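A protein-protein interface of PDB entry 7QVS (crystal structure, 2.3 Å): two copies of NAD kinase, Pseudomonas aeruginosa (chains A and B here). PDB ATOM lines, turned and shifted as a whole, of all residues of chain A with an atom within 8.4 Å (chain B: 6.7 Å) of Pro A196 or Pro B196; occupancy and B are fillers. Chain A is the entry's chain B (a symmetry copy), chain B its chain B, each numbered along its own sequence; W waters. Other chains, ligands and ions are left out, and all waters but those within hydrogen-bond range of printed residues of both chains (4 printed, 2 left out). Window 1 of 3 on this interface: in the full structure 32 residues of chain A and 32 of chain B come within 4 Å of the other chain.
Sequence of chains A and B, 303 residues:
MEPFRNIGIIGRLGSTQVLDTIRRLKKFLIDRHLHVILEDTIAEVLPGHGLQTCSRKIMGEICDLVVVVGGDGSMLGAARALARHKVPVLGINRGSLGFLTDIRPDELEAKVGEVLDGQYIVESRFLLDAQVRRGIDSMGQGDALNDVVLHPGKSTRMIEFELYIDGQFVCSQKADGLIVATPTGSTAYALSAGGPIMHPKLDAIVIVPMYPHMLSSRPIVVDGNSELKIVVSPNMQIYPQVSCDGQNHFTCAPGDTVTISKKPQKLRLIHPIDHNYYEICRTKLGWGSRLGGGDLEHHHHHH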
ATOM      1  N   ALA A 181      11.950 -20.666  16.944  1.00  0.00           N
ATOM      2  CA  ALA A 181      11.219 -21.594  17.805  1.00  0.00           C
ATOM      3  C   ALA A 181      12.083 -22.743  18.319  1.00  0.00           C
ATOM      4  O   ALA A 181      12.953 -23.259  17.618  1.00  0.00           O
ATOM      5  CB  ALA A 181       9.993 -22.173  17.081  1.00  0.00           C
ATOM      6  N   THR A 182      11.817 -23.133  19.555  1.00  0.00           N
ATOM      7  CA  THR A 182      12.308 -24.376  20.128  1.00  0.00           C
ATOM      8  C   THR A 182      11.548 -25.566  19.535  1.00  0.00           C
ATOM      9  O   THR A 182      10.549 -25.389  18.841  1.00  0.00           O
ATOM     10  CB  THR A 182      12.104 -24.351  21.646  1.00  0.00           C
ATOM     11  OG1 THR A 182      10.698 -24.207  21.927  1.00  0.00           O
ATOM     12  CG2 THR A 182      12.895 -23.227  22.296  1.00  0.00           C
ATOM     13  N   PRO A 183      11.976 -26.805  19.827  1.00  0.00           N
ATOM     14  CA  PRO A 183      11.121 -27.963  19.501  1.00  0.00           C
ATOM     15  C   PRO A 183       9.714 -27.866  20.081  1.00  0.00           C
ATOM     16  O   PRO A 183       8.750 -28.216  19.389  1.00  0.00           O
ATOM     17  CB  PRO A 183      11.901 -29.140  20.098  1.00  0.00           C
ATOM     18  CG  PRO A 183      13.307 -28.672  20.062  1.00  0.00           C
ATOM     19  CD  PRO A 183      13.257 -27.238  20.414  1.00  0.00           C
ATOM     20  N   GLY A 185       8.079 -25.057  20.672  1.00  0.00           N
ATOM     21  CA  GLY A 185       7.382 -24.070  19.859  1.00  0.00           C
ATOM     22  C   GLY A 185       7.187 -24.457  18.399  1.00  0.00           C
ATOM     23  O   GLY A 185       6.468 -23.745  17.690  1.00  0.00           O
ATOM     24  N   SER A 186       7.790 -25.562  17.942  1.00  0.00           N
ATOM     25  CA  SER A 186       7.688 -25.936  16.530  1.00  0.00           C
ATOM     26  C   SER A 186       6.257 -26.283  16.115  1.00  0.00           C
ATOM     27  O   SER A 186       5.931 -26.178  14.929  1.00  0.00           O
ATOM     28  CB  SER A 186       8.624 -27.104  16.213  1.00  0.00           C
ATOM     29  OG  SER A 186       8.236 -28.319  16.850  1.00  0.00           O
ATOM     30  N   THR A 187       5.405 -26.681  17.060  1.00  0.00           N
ATOM     31  CA  THR A 187       4.007 -26.973  16.792  1.00  0.00           C
ATOM     32  C   THR A 187       3.083 -25.782  17.033  1.00  0.00           C
ATOM     33  O   THR A 187       1.868 -25.927  16.868  1.00  0.00           O
ATOM     34  CB  THR A 187       3.527 -28.170  17.649  1.00  0.00           C
ATOM     35  OG1 THR A 187       3.832 -27.944  19.028  1.00  0.00           O
ATOM     36  CG2 THR A 187       4.177 -29.454  17.213  1.00  0.00           C
ATOM     37  N   ALA A 188       3.608 -24.618  17.420  1.00  0.00           N
ATOM     38  CA  ALA A 188       2.753 -23.455  17.674  1.00  0.00           C
ATOM     39  C   ALA A 188       2.782 -22.456  16.501  1.00  0.00           C
ATOM     40  O   ALA A 188       2.477 -22.830  15.365  1.00  0.00           O
ATOM     41  CB  ALA A 188       3.164 -22.802  19.005  1.00  0.00           C
ATOM     42  N   ALA A 190       5.216 -21.282  14.662  1.00  0.00           N
ATOM     43  CA  ALA A 190       6.092 -21.715  13.582  1.00  0.00           C
ATOM     44  C   ALA A 190       5.390 -22.704  12.649  1.00  0.00           C
ATOM     45  O   ALA A 190       5.547 -22.629  11.429  1.00  0.00           O
ATOM     46  CB  ALA A 190       7.368 -22.316  14.173  1.00  0.00           C
ATOM     47  N   LEU A 191       4.576 -23.603  13.206  1.00  0.00           N
ATOM     48  CA  LEU A 191       3.859 -24.584  12.396  1.00  0.00           C
ATOM     49  C   LEU A 191       2.833 -23.915  11.477  1.00  0.00           C
ATOM     50  O   LEU A 191       2.756 -24.228  10.282  1.00  0.00           O
ATOM     51  CB  LEU A 191       3.178 -25.612  13.312  1.00  0.00           C
ATOM     52  CG  LEU A 191       2.600 -26.830  12.573  1.00  0.00           C
ATOM     53  CD1 LEU A 191       3.756 -27.676  12.067  1.00  0.00           C
ATOM     54  CD2 LEU A 191       1.654 -27.657  13.441  1.00  0.00           C
ATOM     55  N   SER A 192       2.037 -22.984  12.025  1.00  0.00           N
ATOM     56  CA  SER A 192       1.078 -22.222  11.223  1.00  0.00           C
ATOM     57  C   SER A 192       1.761 -21.432  10.124  1.00  0.00           C
ATOM     58  O   SER A 192       1.169 -21.214   9.060  1.00  0.00           O
ATOM     59  CB  SER A 192       0.288 -21.253  12.099  1.00  0.00           C
ATOM     60  OG  SER A 192      -0.370 -21.959  13.094  1.00  0.00           O
ATOM     61  N   ALA A 193       2.989 -20.971  10.376  1.00  0.00           N
ATOM     62  CA  ALA A 193       3.732 -20.193   9.399  1.00  0.00           C
ATOM     63  C   ALA A 193       4.434 -21.061   8.366  1.00  0.00           C
ATOM     64  O   ALA A 193       5.162 -20.518   7.534  1.00  0.00           O
ATOM     65  CB  ALA A 193       4.758 -19.304  10.108  1.00  0.00           C
ATOM     66  N   GLY A 194       4.266 -22.382   8.414  1.00  0.00           N
ATOM     67  CA  GLY A 194       4.885 -23.267   7.441  1.00  0.00           C
ATOM     68  C   GLY A 194       6.103 -24.033   7.911  1.00  0.00           C
ATOM     69  O   GLY A 194       6.734 -24.721   7.092  1.00  0.00           O
ATOM     70  N   GLY A 195       6.462 -23.947   9.196  1.00  0.00           N
ATOM     71  CA  GLY A 195       7.650 -24.625   9.677  1.00  0.00           C
ATOM     72  C   GLY A 195       7.435 -26.109   9.909  1.00  0.00           C
ATOM     73  O   GLY A 195       6.300 -26.572  10.017  1.00  0.00           O
ATOM     74  N   PRO A 196       8.519 -26.874  10.027  1.00  0.00           N
ATOM     75  CA  PRO A 196       8.399 -28.309  10.326  1.00  0.00           C
ATOM     76  C   PRO A 196       8.164 -28.582  11.806  1.00  0.00           C
ATOM     77  O   PRO A 196       8.514 -27.786  12.684  1.00  0.00           O
ATOM     78  CB  PRO A 196       9.761 -28.858   9.914  1.00  0.00           C
ATOM     79  CG  PRO A 196      10.708 -27.722  10.369  1.00  0.00           C
ATOM     80  CD  PRO A 196       9.926 -26.429  10.054  1.00  0.00           C
ATOM     81  N   ILE A 197       7.581 -29.739  12.077  1.00  0.00           N
ATOM     82  CA  ILE A 197       7.531 -30.244  13.445  1.00  0.00           C
ATOM     83  C   ILE A 197       8.911 -30.777  13.803  1.00  0.00           C
ATOM     84  O   ILE A 197       9.579 -31.403  12.976  1.00  0.00           O
ATOM     85  CB  ILE A 197       6.447 -31.328  13.588  1.00  0.00           C
ATOM     86  CG1 ILE A 197       5.081 -30.780  13.156  1.00  0.00           C
ATOM     87  CG2 ILE A 197       6.388 -31.865  15.019  1.00  0.00           C
ATOM     88  CD1 ILE A 197       4.122 -31.837  12.782  1.00  0.00           C
ATOM     89  N   MET A 198       9.364 -30.482  15.017  1.00  0.00           N
ATOM     90  CA  MET A 198      10.649 -30.949  15.535  1.00  0.00           C
ATOM     91  C   MET A 198      10.372 -31.785  16.774  1.00  0.00           C
ATOM     92  O   MET A 198       9.705 -31.320  17.701  1.00  0.00           O
ATOM     93  CB  MET A 198      11.545 -29.773  15.905  1.00  0.00           C
ATOM     94  CG  MET A 198      11.788 -28.769  14.787  1.00  0.00           C
ATOM     95  SD  MET A 198      13.426 -28.052  14.894  1.00  0.00           S
ATOM     96  CE  MET A 198      13.110 -26.897  16.198  1.00  0.00           C
ATOM     97  N   HIS A 199      10.864 -33.007  16.788  1.00  0.00           N
ATOM     98  CA  HIS A 199      10.618 -33.882  17.923  1.00  0.00           C
ATOM     99  C   HIS A 199      11.118 -33.232  19.219  1.00  0.00           C
ATOM    100  O   HIS A 199      12.179 -32.594  19.222  1.00  0.00           O
ATOM    101  CB  HIS A 199      11.306 -35.222  17.676  1.00  0.00           C
ATOM    102  CG  HIS A 199      11.045 -36.236  18.737  1.00  0.00           C
ATOM    103  ND1 HIS A 199      11.591 -36.155  20.000  1.00  0.00           N
ATOM    104  CD2 HIS A 199      10.274 -37.347  18.731  1.00  0.00           C
ATOM    105  CE1 HIS A 199      11.176 -37.181  20.721  1.00  0.00           C
ATOM    106  NE2 HIS A 199      10.375 -37.919  19.973  1.00  0.00           N
ATOM    107  N   LEU A 202      14.787 -33.335  20.111  1.00  0.00           N
ATOM    108  CA  LEU A 202      15.762 -32.868  19.135  1.00  0.00           C
ATOM    109  C   LEU A 202      16.498 -31.627  19.647  1.00  0.00           C
ATOM    110  O   LEU A 202      15.883 -30.670  20.120  1.00  0.00           O
ATOM    111  CB  LEU A 202      15.067 -32.578  17.811  1.00  0.00           C
ATOM    112  CG  LEU A 202      15.930 -32.277  16.585  1.00  0.00           C
ATOM    113  CD1 LEU A 202      16.613 -33.527  16.111  1.00  0.00           C
ATOM    114  CD2 LEU A 202      15.064 -31.667  15.475  1.00  0.00           C
ATOM    115  N   ILE A 205      16.987 -25.724  16.769  1.00  0.00           N
ATOM    116  CA  ILE A 205      16.186 -24.503  16.747  1.00  0.00           C
ATOM    117  C   ILE A 205      15.747 -24.253  15.308  1.00  0.00           C
ATOM    118  O   ILE A 205      16.564 -24.372  14.384  1.00  0.00           O
ATOM    119  CB  ILE A 205      17.007 -23.302  17.263  1.00  0.00           C
ATOM    120  CG1 ILE A 205      17.387 -23.490  18.730  1.00  0.00           C
ATOM    121  CG2 ILE A 205      16.278 -22.003  17.002  1.00  0.00           C
ATOM    122  CD1 ILE A 205      18.393 -22.419  19.237  1.00  0.00           C
ATOM    123  N   VAL A 206      14.483 -23.873  15.106  1.00  0.00           N
ATOM    124  CA  VAL A 206      13.999 -23.559  13.763  1.00  0.00           C
ATOM    125  C   VAL A 206      13.766 -22.056  13.626  1.00  0.00           C
ATOM    126  O   VAL A 206      13.300 -21.389  14.558  1.00  0.00           O
ATOM    127  CB  VAL A 206      12.734 -24.354  13.379  1.00  0.00           C
ATOM    128  CG1 VAL A 206      11.511 -23.899  14.193  1.00  0.00           C
ATOM    129  CG2 VAL A 206      12.471 -24.200  11.874  1.00  0.00           C
ATOM    130  N   ILE A 207      14.104 -21.533  12.454  1.00  0.00           N
ATOM    131  CA  ILE A 207      13.993 -20.118  12.113  1.00  0.00           C
ATOM    132  C   ILE A 207      13.014 -19.997  10.959  1.00  0.00           C
ATOM    133  O   ILE A 207      13.291 -20.499   9.865  1.00  0.00           O
ATOM    134  CB  ILE A 207      15.358 -19.529  11.728  1.00  0.00           C
ATOM    135  CG1 ILE A 207      16.369 -19.739  12.880  1.00  0.00           C
ATOM    136  CG2 ILE A 207      15.205 -18.060  11.335  1.00  0.00           C
ATOM    137  CD1 ILE A 207      17.835 -19.670  12.454  1.00  0.00           C
ATOM    138  N   VAL A 208      11.879 -19.342  11.198  1.00  0.00           N
ATOM    139  CA  VAL A 208      10.776 -19.327  10.235  1.00  0.00           C
ATOM    140  C   VAL A 208      10.454 -17.890   9.843  1.00  0.00           C
ATOM    141  O   VAL A 208       9.990 -17.108  10.671  1.00  0.00           O
ATOM    142  CB  VAL A 208       9.524 -20.046  10.791  1.00  0.00           C
ATOM    143  CG1 VAL A 208       8.428 -20.130   9.746  1.00  0.00           C
ATOM    144  CG2 VAL A 208       9.865 -21.449  11.298  1.00  0.00           C
ATOM    145  N   ARG A 218      12.798 -19.765   3.067  1.00  0.00           N
ATOM    146  CA  ARG A 218      12.390 -21.070   3.566  1.00  0.00           C
ATOM    147  C   ARG A 218      12.903 -21.207   4.984  1.00  0.00           C
ATOM    148  O   ARG A 218      13.908 -20.586   5.337  1.00  0.00           O
ATOM    149  CB  ARG A 218      12.902 -22.229   2.687  1.00  0.00           C
ATOM    150  CG  ARG A 218      12.172 -22.377   1.342  1.00  0.00           C
ATOM    151  CD  ARG A 218      10.645 -22.536   1.519  1.00  0.00           C
ATOM    152  NE  ARG A 218      10.004 -22.969   0.279  1.00  0.00           N
ATOM    153  CZ  ARG A 218       9.730 -22.163  -0.741  1.00  0.00           C
ATOM    154  NH1 ARG A 218      10.014 -20.866  -0.698  1.00  0.00           N
ATOM    155  NH2 ARG A 218       9.171 -22.669  -1.839  1.00  0.00           N
ATOM    156  N   PRO A 219      12.230 -21.979   5.821  1.00  0.00           N
ATOM    157  CA  PRO A 219      12.727 -22.173   7.188  1.00  0.00           C
ATOM    158  C   PRO A 219      14.079 -22.880   7.205  1.00  0.00           C
ATOM    159  O   PRO A 219      14.416 -23.668   6.312  1.00  0.00           O
ATOM    160  CB  PRO A 219      11.639 -23.031   7.849  1.00  0.00           C
ATOM    161  CG  PRO A 219      10.450 -22.975   6.913  1.00  0.00           C
ATOM    162  CD  PRO A 219      10.999 -22.737   5.554  1.00  0.00           C
ATOM    163  N   ILE A 220      14.858 -22.569   8.229  1.00  0.00           N
ATOM    164  CA  ILE A 220      16.159 -23.186   8.470  1.00  0.00           C
ATOM    165  C   ILE A 220      16.164 -23.808   9.862  1.00  0.00           C
ATOM    166  O   ILE A 220      15.726 -23.192  10.842  1.00  0.00           O
ATOM    167  CB  ILE A 220      17.321 -22.176   8.342  1.00  0.00           C
ATOM    168  CG1 ILE A 220      17.143 -21.283   7.118  1.00  0.00           C
ATOM    169  CG2 ILE A 220      18.666 -22.904   8.281  1.00  0.00           C
ATOM    170  CD1 ILE A 220      18.091 -20.071   7.135  1.00  0.00           C
ATOM    171  N   VAL A 221      16.678 -25.023   9.947  1.00  0.00           N
ATOM    172  CA  VAL A 221      16.875 -25.704  11.221  1.00  0.00           C
ATOM    173  C   VAL A 221      18.370 -25.707  11.506  1.00  0.00           C
ATOM    174  O   VAL A 221      19.169 -26.127  10.659  1.00  0.00           O
ATOM    175  CB  VAL A 221      16.304 -27.136  11.202  1.00  0.00           C
ATOM    176  CG1 VAL A 221      16.421 -27.764  12.577  1.00  0.00           C
ATOM    177  CG2 VAL A 221      14.846 -27.113  10.756  1.00  0.00           C
ATOM    178  N   VAL A 222      18.744 -25.217  12.680  1.00  0.00           N
ATOM    179  CA  VAL A 222      20.137 -25.093  13.097  1.00  0.00           C
ATOM    180  C   VAL A 222      20.345 -25.847  14.406  1.00  0.00           C
ATOM    181  O   VAL A 222      19.398 -26.215  15.107  1.00  0.00           O
ATOM    182  CB  VAL A 222      20.565 -23.617  13.248  1.00  0.00           C
ATOM    183  CG1 VAL A 222      20.461 -22.913  11.918  1.00  0.00           C
ATOM    184  CG2 VAL A 222      19.700 -22.905  14.280  1.00  0.00           C
ATOM    185  N   TYR A 277       4.221 -39.215  22.523  1.00  0.00           N
ATOM    186  CA  TYR A 277       4.306 -37.967  21.776  1.00  0.00           C
ATOM    187  C   TYR A 277       3.579 -38.053  20.431  1.00  0.00           C
ATOM    188  O   TYR A 277       2.875 -37.116  20.038  1.00  0.00           O
ATOM    189  CB  TYR A 277       5.779 -37.591  21.570  1.00  0.00           C
ATOM    190  CG  TYR A 277       5.946 -36.502  20.547  1.00  0.00           C
ATOM    191  CD1 TYR A 277       5.592 -35.206  20.844  1.00  0.00           C
ATOM    192  CD2 TYR A 277       6.420 -36.785  19.271  1.00  0.00           C
ATOM    193  CE1 TYR A 277       5.702 -34.210  19.899  1.00  0.00           C
ATOM    194  CE2 TYR A 277       6.545 -35.804  18.325  1.00  0.00           C
ATOM    195  CZ  TYR A 277       6.188 -34.513  18.647  1.00  0.00           C
ATOM    196  OH  TYR A 277       6.310 -33.519  17.720  1.00  0.00           O
ATOM    197  N   SER B 186      18.355 -31.907   2.218  1.00  0.00           N
ATOM    198  CA  SER B 186      17.306 -30.974   2.630  1.00  0.00           C
ATOM    199  C   SER B 186      17.107 -29.833   1.630  1.00  0.00           C
ATOM    200  O   SER B 186      16.020 -29.250   1.588  1.00  0.00           O
ATOM    201  CB  SER B 186      17.605 -30.406   4.020  1.00  0.00           C
ATOM    202  OG  SER B 186      18.753 -29.560   4.042  1.00  0.00           O
ATOM    203  N   THR B 187      18.122 -29.515   0.826  1.00  0.00           N
ATOM    204  CA  THR B 187      18.024 -28.495  -0.204  1.00  0.00           C
ATOM    205  C   THR B 187      17.648 -29.053  -1.574  1.00  0.00           C
ATOM    206  O   THR B 187      17.569 -28.278  -2.533  1.00  0.00           O
ATOM    207  CB  THR B 187      19.355 -27.711  -0.323  1.00  0.00           C
ATOM    208  OG1 THR B 187      20.449 -28.618  -0.487  1.00  0.00           O
ATOM    209  CG2 THR B 187      19.605 -26.865   0.894  1.00  0.00           C
ATOM    210  N   ALA B 190      13.389 -32.519  -1.048  1.00  0.00           N
ATOM    211  CA  ALA B 190      12.664 -32.159   0.161  1.00  0.00           C
ATOM    212  C   ALA B 190      12.330 -30.667   0.195  1.00  0.00           C
ATOM    213  O   ALA B 190      11.229 -30.282   0.596  1.00  0.00           O
ATOM    214  CB  ALA B 190      13.479 -32.576   1.386  1.00  0.00           C
ATOM    215  N   LEU B 191      13.251 -29.820  -0.268  1.00  0.00           N
ATOM    216  CA  LEU B 191      13.021 -28.377  -0.282  1.00  0.00           C
ATOM    217  C   LEU B 191      11.887 -27.996  -1.238  1.00  0.00           C
ATOM    218  O   LEU B 191      10.997 -27.212  -0.882  1.00  0.00           O
ATOM    219  CB  LEU B 191      14.319 -27.649  -0.662  1.00  0.00           C
ATOM    220  CG  LEU B 191      14.267 -26.125  -0.469  1.00  0.00           C
ATOM    221  CD1 LEU B 191      14.244 -25.831   1.021  1.00  0.00           C
ATOM    222  CD2 LEU B 191      15.424 -25.401  -1.154  1.00  0.00           C
ATOM    223  N   GLY B 194       8.472 -28.565   0.105  1.00  0.00           N
ATOM    224  CA  GLY B 194       8.059 -27.780   1.257  1.00  0.00           C
ATOM    225  C   GLY B 194       8.849 -27.991   2.531  1.00  0.00           C
ATOM    226  O   GLY B 194       8.474 -27.427   3.571  1.00  0.00           O
ATOM    227  N   GLY B 195       9.930 -28.777   2.495  1.00  0.00           N
ATOM    228  CA  GLY B 195      10.686 -29.046   3.703  1.00  0.00           C
ATOM    229  C   GLY B 195      11.614 -27.907   4.088  1.00  0.00           C
ATOM    230  O   GLY B 195      11.928 -27.046   3.269  1.00  0.00           O
ATOM    231  N   PRO B 196      12.096 -27.904   5.330  1.00  0.00           N
ATOM    232  CA  PRO B 196      13.058 -26.879   5.762  1.00  0.00           C
ATOM    233  C   PRO B 196      14.481 -27.184   5.314  1.00  0.00           C
ATOM    234  O   PRO B 196      14.860 -28.334   5.069  1.00  0.00           O
ATOM    235  CB  PRO B 196      12.973 -26.951   7.284  1.00  0.00           C
ATOM    236  CG  PRO B 196      12.819 -28.474   7.517  1.00  0.00           C
ATOM    237  CD  PRO B 196      11.908 -28.942   6.362  1.00  0.00           C
ATOM    238  N   ILE B 197      15.280 -26.132   5.231  1.00  0.00           N
ATOM    239  CA  ILE B 197      16.720 -26.303   5.069  1.00  0.00           C
ATOM    240  C   ILE B 197      17.299 -26.724   6.414  1.00  0.00           C
ATOM    241  O   ILE B 197      16.887 -26.222   7.462  1.00  0.00           O
ATOM    242  CB  ILE B 197      17.369 -25.009   4.550  1.00  0.00           C
ATOM    243  CG1 ILE B 197      16.718 -24.575   3.230  1.00  0.00           C
ATOM    244  CG2 ILE B 197      18.880 -25.178   4.378  1.00  0.00           C
ATOM    245  CD1 ILE B 197      16.904 -23.142   2.933  1.00  0.00           C
ATOM    246  N   MET B 198      18.217 -27.685   6.388  1.00  0.00           N
ATOM    247  CA  MET B 198      18.903 -28.177   7.582  1.00  0.00           C
ATOM    248  C   MET B 198      20.391 -27.930   7.395  1.00  0.00           C
ATOM    249  O   MET B 198      20.969 -28.352   6.390  1.00  0.00           O
ATOM    250  CB  MET B 198      18.655 -29.669   7.774  1.00  0.00           C
ATOM    251  CG  MET B 198      17.190 -30.078   7.832  1.00  0.00           C
ATOM    252  SD  MET B 198      16.941 -31.470   8.930  1.00  0.00           S
ATOM    253  CE  MET B 198      17.513 -32.750   7.849  1.00  0.00           C
ATOM    254  N   VAL B 206      15.088 -35.263   8.028  1.00  0.00           N
ATOM    255  CA  VAL B 206      13.760 -34.695   7.798  1.00  0.00           C
ATOM    256  C   VAL B 206      12.905 -35.669   6.990  1.00  0.00           C
ATOM    257  O   VAL B 206      13.390 -36.345   6.075  1.00  0.00           O
ATOM    258  CB  VAL B 206      13.808 -33.308   7.125  1.00  0.00           C
ATOM    259  CG1 VAL B 206      14.289 -33.403   5.667  1.00  0.00           C
ATOM    260  CG2 VAL B 206      12.419 -32.658   7.195  1.00  0.00           C
ATOM    261  N   VAL B 208       9.452 -35.784   4.781  1.00  0.00           N
ATOM    262  CA  VAL B 208       8.599 -34.849   4.046  1.00  0.00           C
ATOM    263  C   VAL B 208       7.553 -35.619   3.250  1.00  0.00           C
ATOM    264  O   VAL B 208       7.890 -36.341   2.313  1.00  0.00           O
ATOM    265  CB  VAL B 208       9.429 -33.924   3.124  1.00  0.00           C
ATOM    266  CG1 VAL B 208       8.554 -32.881   2.456  1.00  0.00           C
ATOM    267  CG2 VAL B 208      10.558 -33.237   3.894  1.00  0.00           C
ATOM    268  N   ARG B 218       2.569 -32.461   7.734  1.00  0.00           N
ATOM    269  CA  ARG B 218       3.641 -31.478   7.811  1.00  0.00           C
ATOM    270  C   ARG B 218       4.947 -32.226   7.973  1.00  0.00           C
ATOM    271  O   ARG B 218       4.956 -33.341   8.501  1.00  0.00           O
ATOM    272  CB  ARG B 218       3.442 -30.472   8.963  1.00  0.00           C
ATOM    273  CG  ARG B 218       2.339 -29.431   8.715  1.00  0.00           C
ATOM    274  CD  ARG B 218       2.563 -28.639   7.408  1.00  0.00           C
ATOM    275  NE  ARG B 218       1.690 -27.469   7.333  1.00  0.00           N
ATOM    276  CZ  ARG B 218       0.405 -27.517   6.999  1.00  0.00           C
ATOM    277  NH1 ARG B 218      -0.191 -28.663   6.687  1.00  0.00           N
ATOM    278  NH2 ARG B 218      -0.308 -26.392   6.992  1.00  0.00           N
ATOM    279  N   PRO B 219       6.051 -31.665   7.510  1.00  0.00           N
ATOM    280  CA  PRO B 219       7.340 -32.340   7.695  1.00  0.00           C
ATOM    281  C   PRO B 219       7.708 -32.468   9.170  1.00  0.00           C
ATOM    282  O   PRO B 219       7.316 -31.654  10.015  1.00  0.00           O
ATOM    283  CB  PRO B 219       8.332 -31.434   6.949  1.00  0.00           C
ATOM    284  CG  PRO B 219       7.482 -30.498   6.115  1.00  0.00           C
ATOM    285  CD  PRO B 219       6.183 -30.371   6.823  1.00  0.00           C
ATOM    286  N   ILE B 220       8.453 -33.522   9.469  1.00  0.00           N
ATOM    287  CA  ILE B 220       8.971 -33.789  10.807  1.00  0.00           C
ATOM    288  C   ILE B 220      10.490 -33.908  10.739  1.00  0.00           C
ATOM    289  O   ILE B 220      11.040 -34.580   9.857  1.00  0.00           O
ATOM    290  CB  ILE B 220       8.371 -35.072  11.423  1.00  0.00           C
ATOM    291  CG1 ILE B 220       6.866 -35.146  11.186  1.00  0.00           C
ATOM    292  CG2 ILE B 220       8.681 -35.149  12.921  1.00  0.00           C
ATOM    293  CD1 ILE B 220       6.292 -36.542  11.495  1.00  0.00           C
ATOM    294  N   VAL B 221      11.160 -33.270  11.682  1.00  0.00           N
ATOM    295  CA  VAL B 221      12.605 -33.387  11.834  1.00  0.00           C
ATOM    296  C   VAL B 221      12.862 -34.237  13.071  1.00  0.00           C
ATOM    297  O   VAL B 221      12.332 -33.948  14.151  1.00  0.00           O
ATOM    298  CB  VAL B 221      13.285 -32.010  11.949  1.00  0.00           C
ATOM    299  CG1 VAL B 221      14.793 -32.171  11.984  1.00  0.00           C
ATOM    300  CG2 VAL B 221      12.878 -31.125  10.774  1.00  0.00           C
HETATM  301  O   HOH W   1       8.977 -25.432  -1.734  1.00  0.00           O
HETATM  302  O   HOH W   2       3.751 -26.104   8.718  1.00  0.00           O
HETATM  303  O   HOH W   3      10.554 -25.605   1.161  1.00  0.00           O
HETATM  304  O   HOH W   4       1.133 -24.235   7.970  1.00  0.00           O
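The side-chain hydroxyl (OG) of Ser A186 lies within hydrogen-bond range of the backbone NH (N) of Met A198, 3.1 Å away. The backbone NH (N) of Ile A207 lies within hydrogen-bond range of the backbone carbonyl oxygen (O) of Ile A220, at 2.8 Å. OG of Ser B186 sits at hydrogen-bond distance from N of Met B198 (3.1 Å).
Of the 28 printed residues of chain A, 8 touch a printed residue of chain B. Hydrophobic or aromatic side chains of chain B within 4 Å of the printed part of chain A: Pro B196, Ile B197, Ile B220 and Val B221.
Pro A196 touches Pro B219, and with the chains exchanged Pro A219 touches Pro B196. Ile A197 touches Pro B219, and with the chains exchanged Pro A219 touches Ile B197. Met A198 touches Val B221, and with the chains exchanged Val A221 touches Met B198. Positions printed for both chains: 186, 187, 190, 191, 194, 195, 196, 197, 198, 206, 208, 218, 219, 220 and 221.
Thr A187 touches none of the printed residues of chain B. Gly A194 touches none of the printed residues of chain B. Of chain B, only Pro B196 (3.6 Å), Pro B219 (3.5 Å) and Val B221 (3.9 Å) come within 4 Å of Pro A196. Of the printed residues of chain B, His A199 touches Val B221 (3.2 Å). Of the printed residues of chain B, Pro A219 touches Pro B196 (3.5 Å) and Ile B197 (2.8 Å). Printed residues of chain B within 4 Å of Ile A220: Ile B197 (3.3 Å). Of the printed residues of chain A, Pro B196 touches Pro A196, Pro A219 and Val A221.
Water W2 lies within hydrogen-bond range of O of Leu A191 (2.6 Å), NE of Arg B218 (2.8 Å) and O of Gly A195 (2.9 Å). Water W1 lies within hydrogen-bond range of NH2 of Arg A218 (2.8 Å) and O of Leu B191 (2.8 Å). Water W4 lies within hydrogen-bond range of the guanidinium group of Arg B218 (2.8 Å), the backbone carbonyl oxygen of Leu A191 (2.8 Å) and the backbone carbonyl oxygen of Ser A192 (3.2 Å).
The backbone NH (N) of His A199 lies within hydrogen-bond range of the backbone carbonyl oxygen (O) of Val B221, 3.2 Å away. O of Ile B197 lies within hydrogen-bond range of N of Val A221 (2.8 Å). The backbone NH (N) of Val B221 lies within hydrogen-bond range of the backbone carbonyl oxygen (O) of Ile A197 (2.8 Å). The backbone NH of Ile B197 lies within hydrogen-bond range of the backbone carbonyl oxygen of Pro A219. The backbone carbonyl oxygen of Pro B219 is in hydrogen-bond range of the backbone NH of Ile A197 (2.8 Å).
Among the printed residues, pairs that only touch across the chains: Pro A196 with Pro B196 (3.6 Å), Pro A196 with Pro B219 (3.5 Å), Pro A196 with Val B221 (3.9 Å), Ile A197 with Ile B220 (3.3 Å), Met A198 with Val B221 (3.7 Å), Leu A202 with Val B221 (3.5 Å), Pro A219 with Pro B196 (3.5 Å), Ile A220 with Ile B197 (3.3 Å), Val A221 with Pro B196 (3.9 Å) and Val A221 with Met B198 (3.7 Å).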
